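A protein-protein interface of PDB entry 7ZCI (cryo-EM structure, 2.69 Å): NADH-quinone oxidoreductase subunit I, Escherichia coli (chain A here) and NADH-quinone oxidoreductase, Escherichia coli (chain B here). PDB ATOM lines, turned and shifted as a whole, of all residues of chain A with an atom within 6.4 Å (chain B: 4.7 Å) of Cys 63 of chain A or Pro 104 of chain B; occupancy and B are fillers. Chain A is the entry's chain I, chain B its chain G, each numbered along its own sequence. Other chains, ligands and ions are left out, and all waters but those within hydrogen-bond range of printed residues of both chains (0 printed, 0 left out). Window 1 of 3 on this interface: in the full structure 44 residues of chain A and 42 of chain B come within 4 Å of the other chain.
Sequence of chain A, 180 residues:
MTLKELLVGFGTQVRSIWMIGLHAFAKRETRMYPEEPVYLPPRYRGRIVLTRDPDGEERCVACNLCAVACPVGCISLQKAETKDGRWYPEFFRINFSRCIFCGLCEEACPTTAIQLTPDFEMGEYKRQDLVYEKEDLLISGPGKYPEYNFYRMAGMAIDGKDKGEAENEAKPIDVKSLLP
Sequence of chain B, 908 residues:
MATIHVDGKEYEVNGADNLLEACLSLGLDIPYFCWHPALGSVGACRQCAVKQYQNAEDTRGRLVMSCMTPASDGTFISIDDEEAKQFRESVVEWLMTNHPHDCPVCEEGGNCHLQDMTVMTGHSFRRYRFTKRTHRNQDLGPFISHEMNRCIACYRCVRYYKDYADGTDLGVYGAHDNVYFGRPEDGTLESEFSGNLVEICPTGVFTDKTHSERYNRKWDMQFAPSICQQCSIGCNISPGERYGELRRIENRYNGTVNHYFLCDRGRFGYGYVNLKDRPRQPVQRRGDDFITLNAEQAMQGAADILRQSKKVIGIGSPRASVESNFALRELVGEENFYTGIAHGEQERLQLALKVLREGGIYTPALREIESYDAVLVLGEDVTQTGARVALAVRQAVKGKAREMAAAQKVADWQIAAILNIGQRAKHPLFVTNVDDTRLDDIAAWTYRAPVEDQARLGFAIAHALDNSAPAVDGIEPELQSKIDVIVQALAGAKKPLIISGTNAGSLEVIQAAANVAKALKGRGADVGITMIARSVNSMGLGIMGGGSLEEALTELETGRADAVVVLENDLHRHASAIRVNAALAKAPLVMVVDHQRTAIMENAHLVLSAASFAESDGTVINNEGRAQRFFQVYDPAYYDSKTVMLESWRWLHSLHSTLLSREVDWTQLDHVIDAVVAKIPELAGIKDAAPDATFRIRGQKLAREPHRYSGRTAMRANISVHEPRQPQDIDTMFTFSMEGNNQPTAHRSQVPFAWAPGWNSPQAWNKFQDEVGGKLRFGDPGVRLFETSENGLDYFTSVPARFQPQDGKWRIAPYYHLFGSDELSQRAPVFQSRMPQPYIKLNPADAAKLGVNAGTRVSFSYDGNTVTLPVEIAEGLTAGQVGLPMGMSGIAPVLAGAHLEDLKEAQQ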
ATOM      1  N   CYS A  60      -6.335 -15.237  25.561  1.00  0.00           N
ATOM      2  CA  CYS A  60      -5.099 -15.003  26.292  1.00  0.00           C
ATOM      3  C   CYS A  60      -4.375 -16.309  26.561  1.00  0.00           C
ATOM      4  O   CYS A  60      -4.970 -17.287  27.016  1.00  0.00           O
ATOM      5  CB  CYS A  60      -5.367 -14.271  27.604  1.00  0.00           C
ATOM      6  SG  CYS A  60      -3.894 -14.009  28.600  1.00  0.00           S
ATOM      7  N   VAL A  61      -3.083 -16.319  26.270  1.00  0.00           N
ATOM      8  CA  VAL A  61      -2.231 -17.470  26.492  1.00  0.00           C
ATOM      9  C   VAL A  61      -1.282 -17.235  27.652  1.00  0.00           C
ATOM     10  O   VAL A  61      -0.350 -18.018  27.851  1.00  0.00           O
ATOM     11  CB  VAL A  61      -1.463 -17.836  25.219  1.00  0.00           C
ATOM     12  CG1 VAL A  61      -2.421 -18.202  24.126  1.00  0.00           C
ATOM     13  CG2 VAL A  61      -0.591 -16.680  24.784  1.00  0.00           C
ATOM     14  N   ALA A  62      -1.490 -16.153  28.402  1.00  0.00           N
ATOM     15  CA  ALA A  62      -0.705 -15.804  29.583  1.00  0.00           C
ATOM     16  C   ALA A  62       0.785 -15.697  29.271  1.00  0.00           C
ATOM     17  O   ALA A  62       1.637 -16.216  29.988  1.00  0.00           O
ATOM     18  CB  ALA A  62      -0.962 -16.781  30.725  1.00  0.00           C
ATOM     19  N   CYS A  63       1.092 -15.022  28.175  1.00  0.00           N
ATOM     20  CA  CYS A  63       2.471 -14.859  27.757  1.00  0.00           C
ATOM     21  C   CYS A  63       3.190 -13.730  28.484  1.00  0.00           C
ATOM     22  O   CYS A  63       4.403 -13.589  28.310  1.00  0.00           O
ATOM     23  CB  CYS A  63       2.512 -14.635  26.250  1.00  0.00           C
ATOM     24  SG  CYS A  63       2.146 -12.988  25.686  1.00  0.00           S
ATOM     25  N   ASN A  64       2.467 -12.916  29.259  1.00  0.00           N
ATOM     26  CA  ASN A  64       3.002 -11.875  30.136  1.00  0.00           C
ATOM     27  C   ASN A  64       3.686 -10.730  29.391  1.00  0.00           C
ATOM     28  O   ASN A  64       4.416  -9.955  30.005  1.00  0.00           O
ATOM     29  CB  ASN A  64       3.960 -12.460  31.183  1.00  0.00           C
ATOM     30  CG  ASN A  64       3.361 -12.499  32.564  1.00  0.00           C
ATOM     31  OD1 ASN A  64       3.287 -11.483  33.243  1.00  0.00           O
ATOM     32  ND2 ASN A  64       2.923 -13.674  32.990  1.00  0.00           N
ATOM     33  N   LEU A  65       3.444 -10.572  28.091  1.00  0.00           N
ATOM     34  CA  LEU A  65       4.023  -9.442  27.374  1.00  0.00           C
ATOM     35  C   LEU A  65       3.335  -8.131  27.735  1.00  0.00           C
ATOM     36  O   LEU A  65       3.995  -7.087  27.802  1.00  0.00           O
ATOM     37  CB  LEU A  65       3.958  -9.688  25.872  1.00  0.00           C
ATOM     38  CG  LEU A  65       4.955 -10.700  25.313  1.00  0.00           C
ATOM     39  CD1 LEU A  65       4.856 -10.724  23.811  1.00  0.00           C
ATOM     40  CD2 LEU A  65       6.375 -10.398  25.771  1.00  0.00           C
ATOM     41  N   CYS A  66       2.028  -8.164  27.996  1.00  0.00           N
ATOM     42  CA  CYS A  66       1.309  -6.951  28.372  1.00  0.00           C
ATOM     43  C   CYS A  66       1.768  -6.414  29.719  1.00  0.00           C
ATOM     44  O   CYS A  66       1.816  -5.198  29.918  1.00  0.00           O
ATOM     45  CB  CYS A  66      -0.194  -7.213  28.407  1.00  0.00           C
ATOM     46  SG  CYS A  66      -0.731  -8.561  29.470  1.00  0.00           S
ATOM     47  N   LEU A  77      -0.696 -11.440  36.135  1.00  0.00           N
ATOM     48  CA  LEU A  77      -1.326 -12.663  35.669  1.00  0.00           C
ATOM     49  C   LEU A  77      -0.385 -13.834  35.905  1.00  0.00           C
ATOM     50  O   LEU A  77       0.811 -13.654  36.138  1.00  0.00           O
ATOM     51  CB  LEU A  77      -1.692 -12.557  34.189  1.00  0.00           C
ATOM     52  CG  LEU A  77      -0.473 -12.349  33.299  1.00  0.00           C
ATOM     53  CD1 LEU A  77      -0.422 -13.423  32.266  1.00  0.00           C
ATOM     54  CD2 LEU A  77      -0.489 -10.982  32.658  1.00  0.00           C
ATOM     55  N   LYS A  79       0.441 -17.913  34.390  1.00  0.00           N
ATOM     56  CA  LYS A  79       0.202 -18.922  33.370  1.00  0.00           C
ATOM     57  C   LYS A  79      -0.310 -20.218  33.989  1.00  0.00           C
ATOM     58  O   LYS A  79       0.223 -20.694  34.994  1.00  0.00           O
ATOM     59  CB  LYS A  79       1.482 -19.176  32.582  1.00  0.00           C
ATOM     60  CG  LYS A  79       1.362 -20.246  31.525  1.00  0.00           C
ATOM     61  CD  LYS A  79       2.135 -21.487  31.902  1.00  0.00           C
ATOM     62  CE  LYS A  79       1.713 -22.663  31.071  1.00  0.00           C
ATOM     63  NZ  LYS A  79       2.456 -23.891  31.405  1.00  0.00           N
ATOM     64  N   TRP A  87      -2.159 -22.976  26.913  1.00  0.00           N
ATOM     65  CA  TRP A  87      -1.842 -21.965  27.909  1.00  0.00           C
ATOM     66  C   TRP A  87      -3.001 -20.988  28.045  1.00  0.00           C
ATOM     67  O   TRP A  87      -3.588 -20.559  27.051  1.00  0.00           O
ATOM     68  CB  TRP A  87      -0.586 -21.188  27.529  1.00  0.00           C
ATOM     69  CG  TRP A  87       0.716 -21.908  27.602  1.00  0.00           C
ATOM     70  CD1 TRP A  87       0.930 -23.236  27.427  1.00  0.00           C
ATOM     71  CD2 TRP A  87       2.004 -21.320  27.810  1.00  0.00           C
ATOM     72  NE1 TRP A  87       2.262 -23.518  27.531  1.00  0.00           N
ATOM     73  CE2 TRP A  87       2.945 -22.357  27.767  1.00  0.00           C
ATOM     74  CE3 TRP A  87       2.449 -20.016  28.049  1.00  0.00           C
ATOM     75  CZ2 TRP A  87       4.301 -22.137  27.954  1.00  0.00           C
ATOM     76  CZ3 TRP A  87       3.792 -19.800  28.225  1.00  0.00           C
ATOM     77  CH2 TRP A  87       4.704 -20.853  28.186  1.00  0.00           C
ATOM     78  N   ALA A 108       1.122  -4.516  22.725  1.00  0.00           N
ATOM     79  CA  ALA A 108       2.076  -5.577  23.007  1.00  0.00           C
ATOM     80  C   ALA A 108       1.481  -6.971  22.899  1.00  0.00           C
ATOM     81  O   ALA A 108       2.242  -7.936  22.839  1.00  0.00           O
ATOM     82  CB  ALA A 108       2.650  -5.409  24.406  1.00  0.00           C
ATOM     83  N   CYS A 109       0.166  -7.102  22.869  1.00  0.00           N
ATOM     84  CA  CYS A 109      -0.453  -8.422  22.890  1.00  0.00           C
ATOM     85  C   CYS A 109      -0.258  -9.155  21.573  1.00  0.00           C
ATOM     86  O   CYS A 109      -0.705  -8.667  20.533  1.00  0.00           O
ATOM     87  CB  CYS A 109      -1.931  -8.312  23.196  1.00  0.00           C
ATOM     88  SG  CYS A 109      -2.770  -9.870  23.491  1.00  0.00           S
ATOM     89  N   PRO A 110       0.378 -10.327  21.570  1.00  0.00           N
ATOM     90  CA  PRO A 110       0.583 -11.062  20.322  1.00  0.00           C
ATOM     91  C   PRO A 110      -0.590 -11.938  19.921  1.00  0.00           C
ATOM     92  O   PRO A 110      -0.505 -12.633  18.909  1.00  0.00           O
ATOM     93  CB  PRO A 110       1.812 -11.910  20.649  1.00  0.00           C
ATOM     94  CG  PRO A 110       1.649 -12.210  22.082  1.00  0.00           C
ATOM     95  CD  PRO A 110       0.988 -11.024  22.713  1.00  0.00           C
ATOM     96  N   THR A 111      -1.667 -11.950  20.697  1.00  0.00           N
ATOM     97  CA  THR A 111      -2.850 -12.722  20.366  1.00  0.00           C
ATOM     98  C   THR A 111      -4.088 -11.855  20.212  1.00  0.00           C
ATOM     99  O   THR A 111      -5.168 -12.392  19.955  1.00  0.00           O
ATOM    100  CB  THR A 111      -3.108 -13.796  21.434  1.00  0.00           C
ATOM    101  OG1 THR A 111      -3.745 -13.210  22.567  1.00  0.00           O
ATOM    102  CG2 THR A 111      -1.823 -14.452  21.890  1.00  0.00           C
ATOM    103  N   PHE A 150      -4.598 -16.876  17.562  1.00  0.00           N
ATOM    104  CA  PHE A 150      -3.167 -17.115  17.678  1.00  0.00           C
ATOM    105  C   PHE A 150      -2.855 -18.598  17.603  1.00  0.00           C
ATOM    106  O   PHE A 150      -1.826 -18.983  17.042  1.00  0.00           O
ATOM    107  CB  PHE A 150      -2.628 -16.527  18.980  1.00  0.00           C
ATOM    108  CG  PHE A 150      -1.289 -17.081  19.390  1.00  0.00           C
ATOM    109  CD1 PHE A 150      -0.129 -16.654  18.774  1.00  0.00           C
ATOM    110  CD2 PHE A 150      -1.192 -18.038  20.384  1.00  0.00           C
ATOM    111  CE1 PHE A 150       1.094 -17.164  19.143  1.00  0.00           C
ATOM    112  CE2 PHE A 150       0.030 -18.554  20.747  1.00  0.00           C
ATOM    113  CZ  PHE A 150       1.172 -18.110  20.133  1.00  0.00           C
ATOM    114  N   ASP B 102       5.818 -19.646  18.010  1.00  0.00           N
ATOM    115  CA  ASP B 102       5.573 -20.224  19.320  1.00  0.00           C
ATOM    116  C   ASP B 102       5.991 -19.370  20.501  1.00  0.00           C
ATOM    117  O   ASP B 102       5.655 -19.743  21.626  1.00  0.00           O
ATOM    118  CB  ASP B 102       6.277 -21.585  19.443  1.00  0.00           C
ATOM    119  CG  ASP B 102       5.357 -22.742  19.174  1.00  0.00           C
ATOM    120  OD1 ASP B 102       4.182 -22.508  18.855  1.00  0.00           O
ATOM    121  OD2 ASP B 102       5.810 -23.894  19.276  1.00  0.00           O
ATOM    122  N   CYS B 103       6.663 -18.236  20.282  1.00  0.00           N
ATOM    123  CA  CYS B 103       7.248 -17.445  21.369  1.00  0.00           C
ATOM    124  C   CYS B 103       6.317 -17.112  22.538  1.00  0.00           C
ATOM    125  O   CYS B 103       6.784 -17.199  23.685  1.00  0.00           O
ATOM    126  CB  CYS B 103       7.841 -16.138  20.814  1.00  0.00           C
ATOM    127  SG  CYS B 103       9.197 -16.280  19.672  1.00  0.00           S
ATOM    128  N   PRO B 104       5.040 -16.728  22.350  1.00  0.00           N
ATOM    129  CA  PRO B 104       4.174 -16.511  23.521  1.00  0.00           C
ATOM    130  C   PRO B 104       3.915 -17.743  24.375  1.00  0.00           C
ATOM    131  O   PRO B 104       3.754 -17.615  25.592  1.00  0.00           O
ATOM    132  CB  PRO B 104       2.876 -15.998  22.890  1.00  0.00           C
ATOM    133  CG  PRO B 104       3.274 -15.435  21.644  1.00  0.00           C
ATOM    134  CD  PRO B 104       4.333 -16.308  21.128  1.00  0.00           C
ATOM    135  N   VAL B 105       3.881 -18.931  23.788  1.00  0.00           N
ATOM    136  CA  VAL B 105       3.509 -20.126  24.535  1.00  0.00           C
ATOM    137  C   VAL B 105       4.734 -21.014  24.684  1.00  0.00           C
ATOM    138  O   VAL B 105       4.633 -22.241  24.751  1.00  0.00           O
ATOM    139  CB  VAL B 105       2.347 -20.866  23.853  1.00  0.00           C
ATOM    140  CG1 VAL B 105       1.077 -20.131  24.088  1.00  0.00           C
ATOM    141  CG2 VAL B 105       2.591 -20.998  22.372  1.00  0.00           C
ATOM    142  N   CYS B 106       5.901 -20.392  24.720  1.00  0.00           N
ATOM    143  CA  CYS B 106       7.174 -21.084  24.797  1.00  0.00           C
ATOM    144  C   CYS B 106       7.868 -20.672  26.080  1.00  0.00           C
ATOM    145  O   CYS B 106       8.003 -19.478  26.358  1.00  0.00           O
ATOM    146  CB  CYS B 106       8.035 -20.747  23.590  1.00  0.00           C
ATOM    147  SG  CYS B 106       9.667 -21.452  23.555  1.00  0.00           S
ATOM    148  N   ARG B 217       8.097 -15.515  33.299  1.00  0.00           N
ATOM    149  CA  ARG B 217       9.192 -15.090  32.447  1.00  0.00           C
ATOM    150  C   ARG B 217      10.359 -14.565  33.275  1.00  0.00           C
ATOM    151  O   ARG B 217      10.207 -14.188  34.436  1.00  0.00           O
ATOM    152  CB  ARG B 217       8.715 -14.023  31.480  1.00  0.00           C
ATOM    153  CG  ARG B 217       7.527 -14.439  30.668  1.00  0.00           C
ATOM    154  CD  ARG B 217       7.941 -14.941  29.322  1.00  0.00           C
ATOM    155  NE  ARG B 217       6.780 -15.311  28.532  1.00  0.00           N
ATOM    156  CZ  ARG B 217       6.769 -16.272  27.623  1.00  0.00           C
ATOM    157  NH1 ARG B 217       7.852 -16.965  27.341  1.00  0.00           N
ATOM    158  NH2 ARG B 217       5.637 -16.555  26.993  1.00  0.00           N
ATOM    159  N   TRP B 219      12.097 -11.876  33.259  1.00  0.00           N
ATOM    160  CA  TRP B 219      12.024 -10.529  33.801  1.00  0.00           C
ATOM    161  C   TRP B 219      11.144 -10.453  35.039  1.00  0.00           C
ATOM    162  O   TRP B 219      11.324  -9.551  35.853  1.00  0.00           O
ATOM    163  CB  TRP B 219      11.532  -9.551  32.735  1.00  0.00           C
ATOM    164  CG  TRP B 219      10.235  -9.933  32.094  1.00  0.00           C
ATOM    165  CD1 TRP B 219       8.989  -9.791  32.618  1.00  0.00           C
ATOM    166  CD2 TRP B 219      10.060 -10.501  30.795  1.00  0.00           C
ATOM    167  NE1 TRP B 219       8.049 -10.245  31.735  1.00  0.00           N
ATOM    168  CE2 TRP B 219       8.681 -10.681  30.602  1.00  0.00           C
ATOM    169  CE3 TRP B 219      10.935 -10.865  29.773  1.00  0.00           C
ATOM    170  CZ2 TRP B 219       8.157 -11.219  29.435  1.00  0.00           C
ATOM    171  CZ3 TRP B 219      10.414 -11.405  28.626  1.00  0.00           C
ATOM    172  CH2 TRP B 219       9.038 -11.573  28.461  1.00  0.00           C
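Of chain B, only Pro 104 (3.3 Å) and Arg 217 (2.9 Å) come within 4 Å of Cys 63 of chain A. Cys 66 of chain A touches none of the printed residues of chain B. Printed residues of chain B within 4 Å of Trp 87 of chain A: Pro 104, Val 105, Cys 106 and Arg 217. Ala 108 of chain A touches none of the printed residues of chain B. Of the printed residues of chain B, Pro 110 of chain A touches Pro 104 (3.6 Å). Of the printed residues of chain A, Pro 104 of chain B touches Cys 63, Trp 87, Pro 110 and Phe 150.
Among the printed residues, merely in contact across the chains: Val 61 of chain A with Val 105 of chain B, Cys 63 of chain A with Pro 104 of chain B, Asn 64 of chain A with Trp 219 of chain B, Leu 65 of chain A with Trp 219 of chain B, Trp 87 of chain A with Pro 104 of chain B, Trp 87 of chain A with Val 105 of chain B, Trp 87 of chain A with Cys 106 of chain B, Trp 87 of chain A with Arg 217 of chain B, Pro 110 of chain A with Pro 104 of chain B, Phe 150 of chain A with Pro 104 of chain B and Phe 150 of chain A with Val 105 of chain B.
The guanidinium group of Arg 217 of chain B sits at hydrogen-bond distance from the backbone carbonyl oxygen of Cys 106 of chain B (2.7 Å). SG of Cys 63 of chain A lies close to N of Leu 65 of chain A (3.6 Å). The backbone carbonyl oxygen of Pro 104 of chain B is in hydrogen-bond range of the guanidinium group of Arg 217 of chain B, 2.6 Å away.
Hydrophobic or aromatic side chains of chain A that line the printed part of chain B: Val 61, Leu 65, Trp 87, Pro 110 and Phe 150. Among the printed residues, 12 pairs touch across the chains.
The guanidinium group (NE) of Arg 217 of chain B lies within hydrogen-bond range of the backbone carbonyl oxygen (O) of Cys 63 of chain A, 2.9 Å away.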
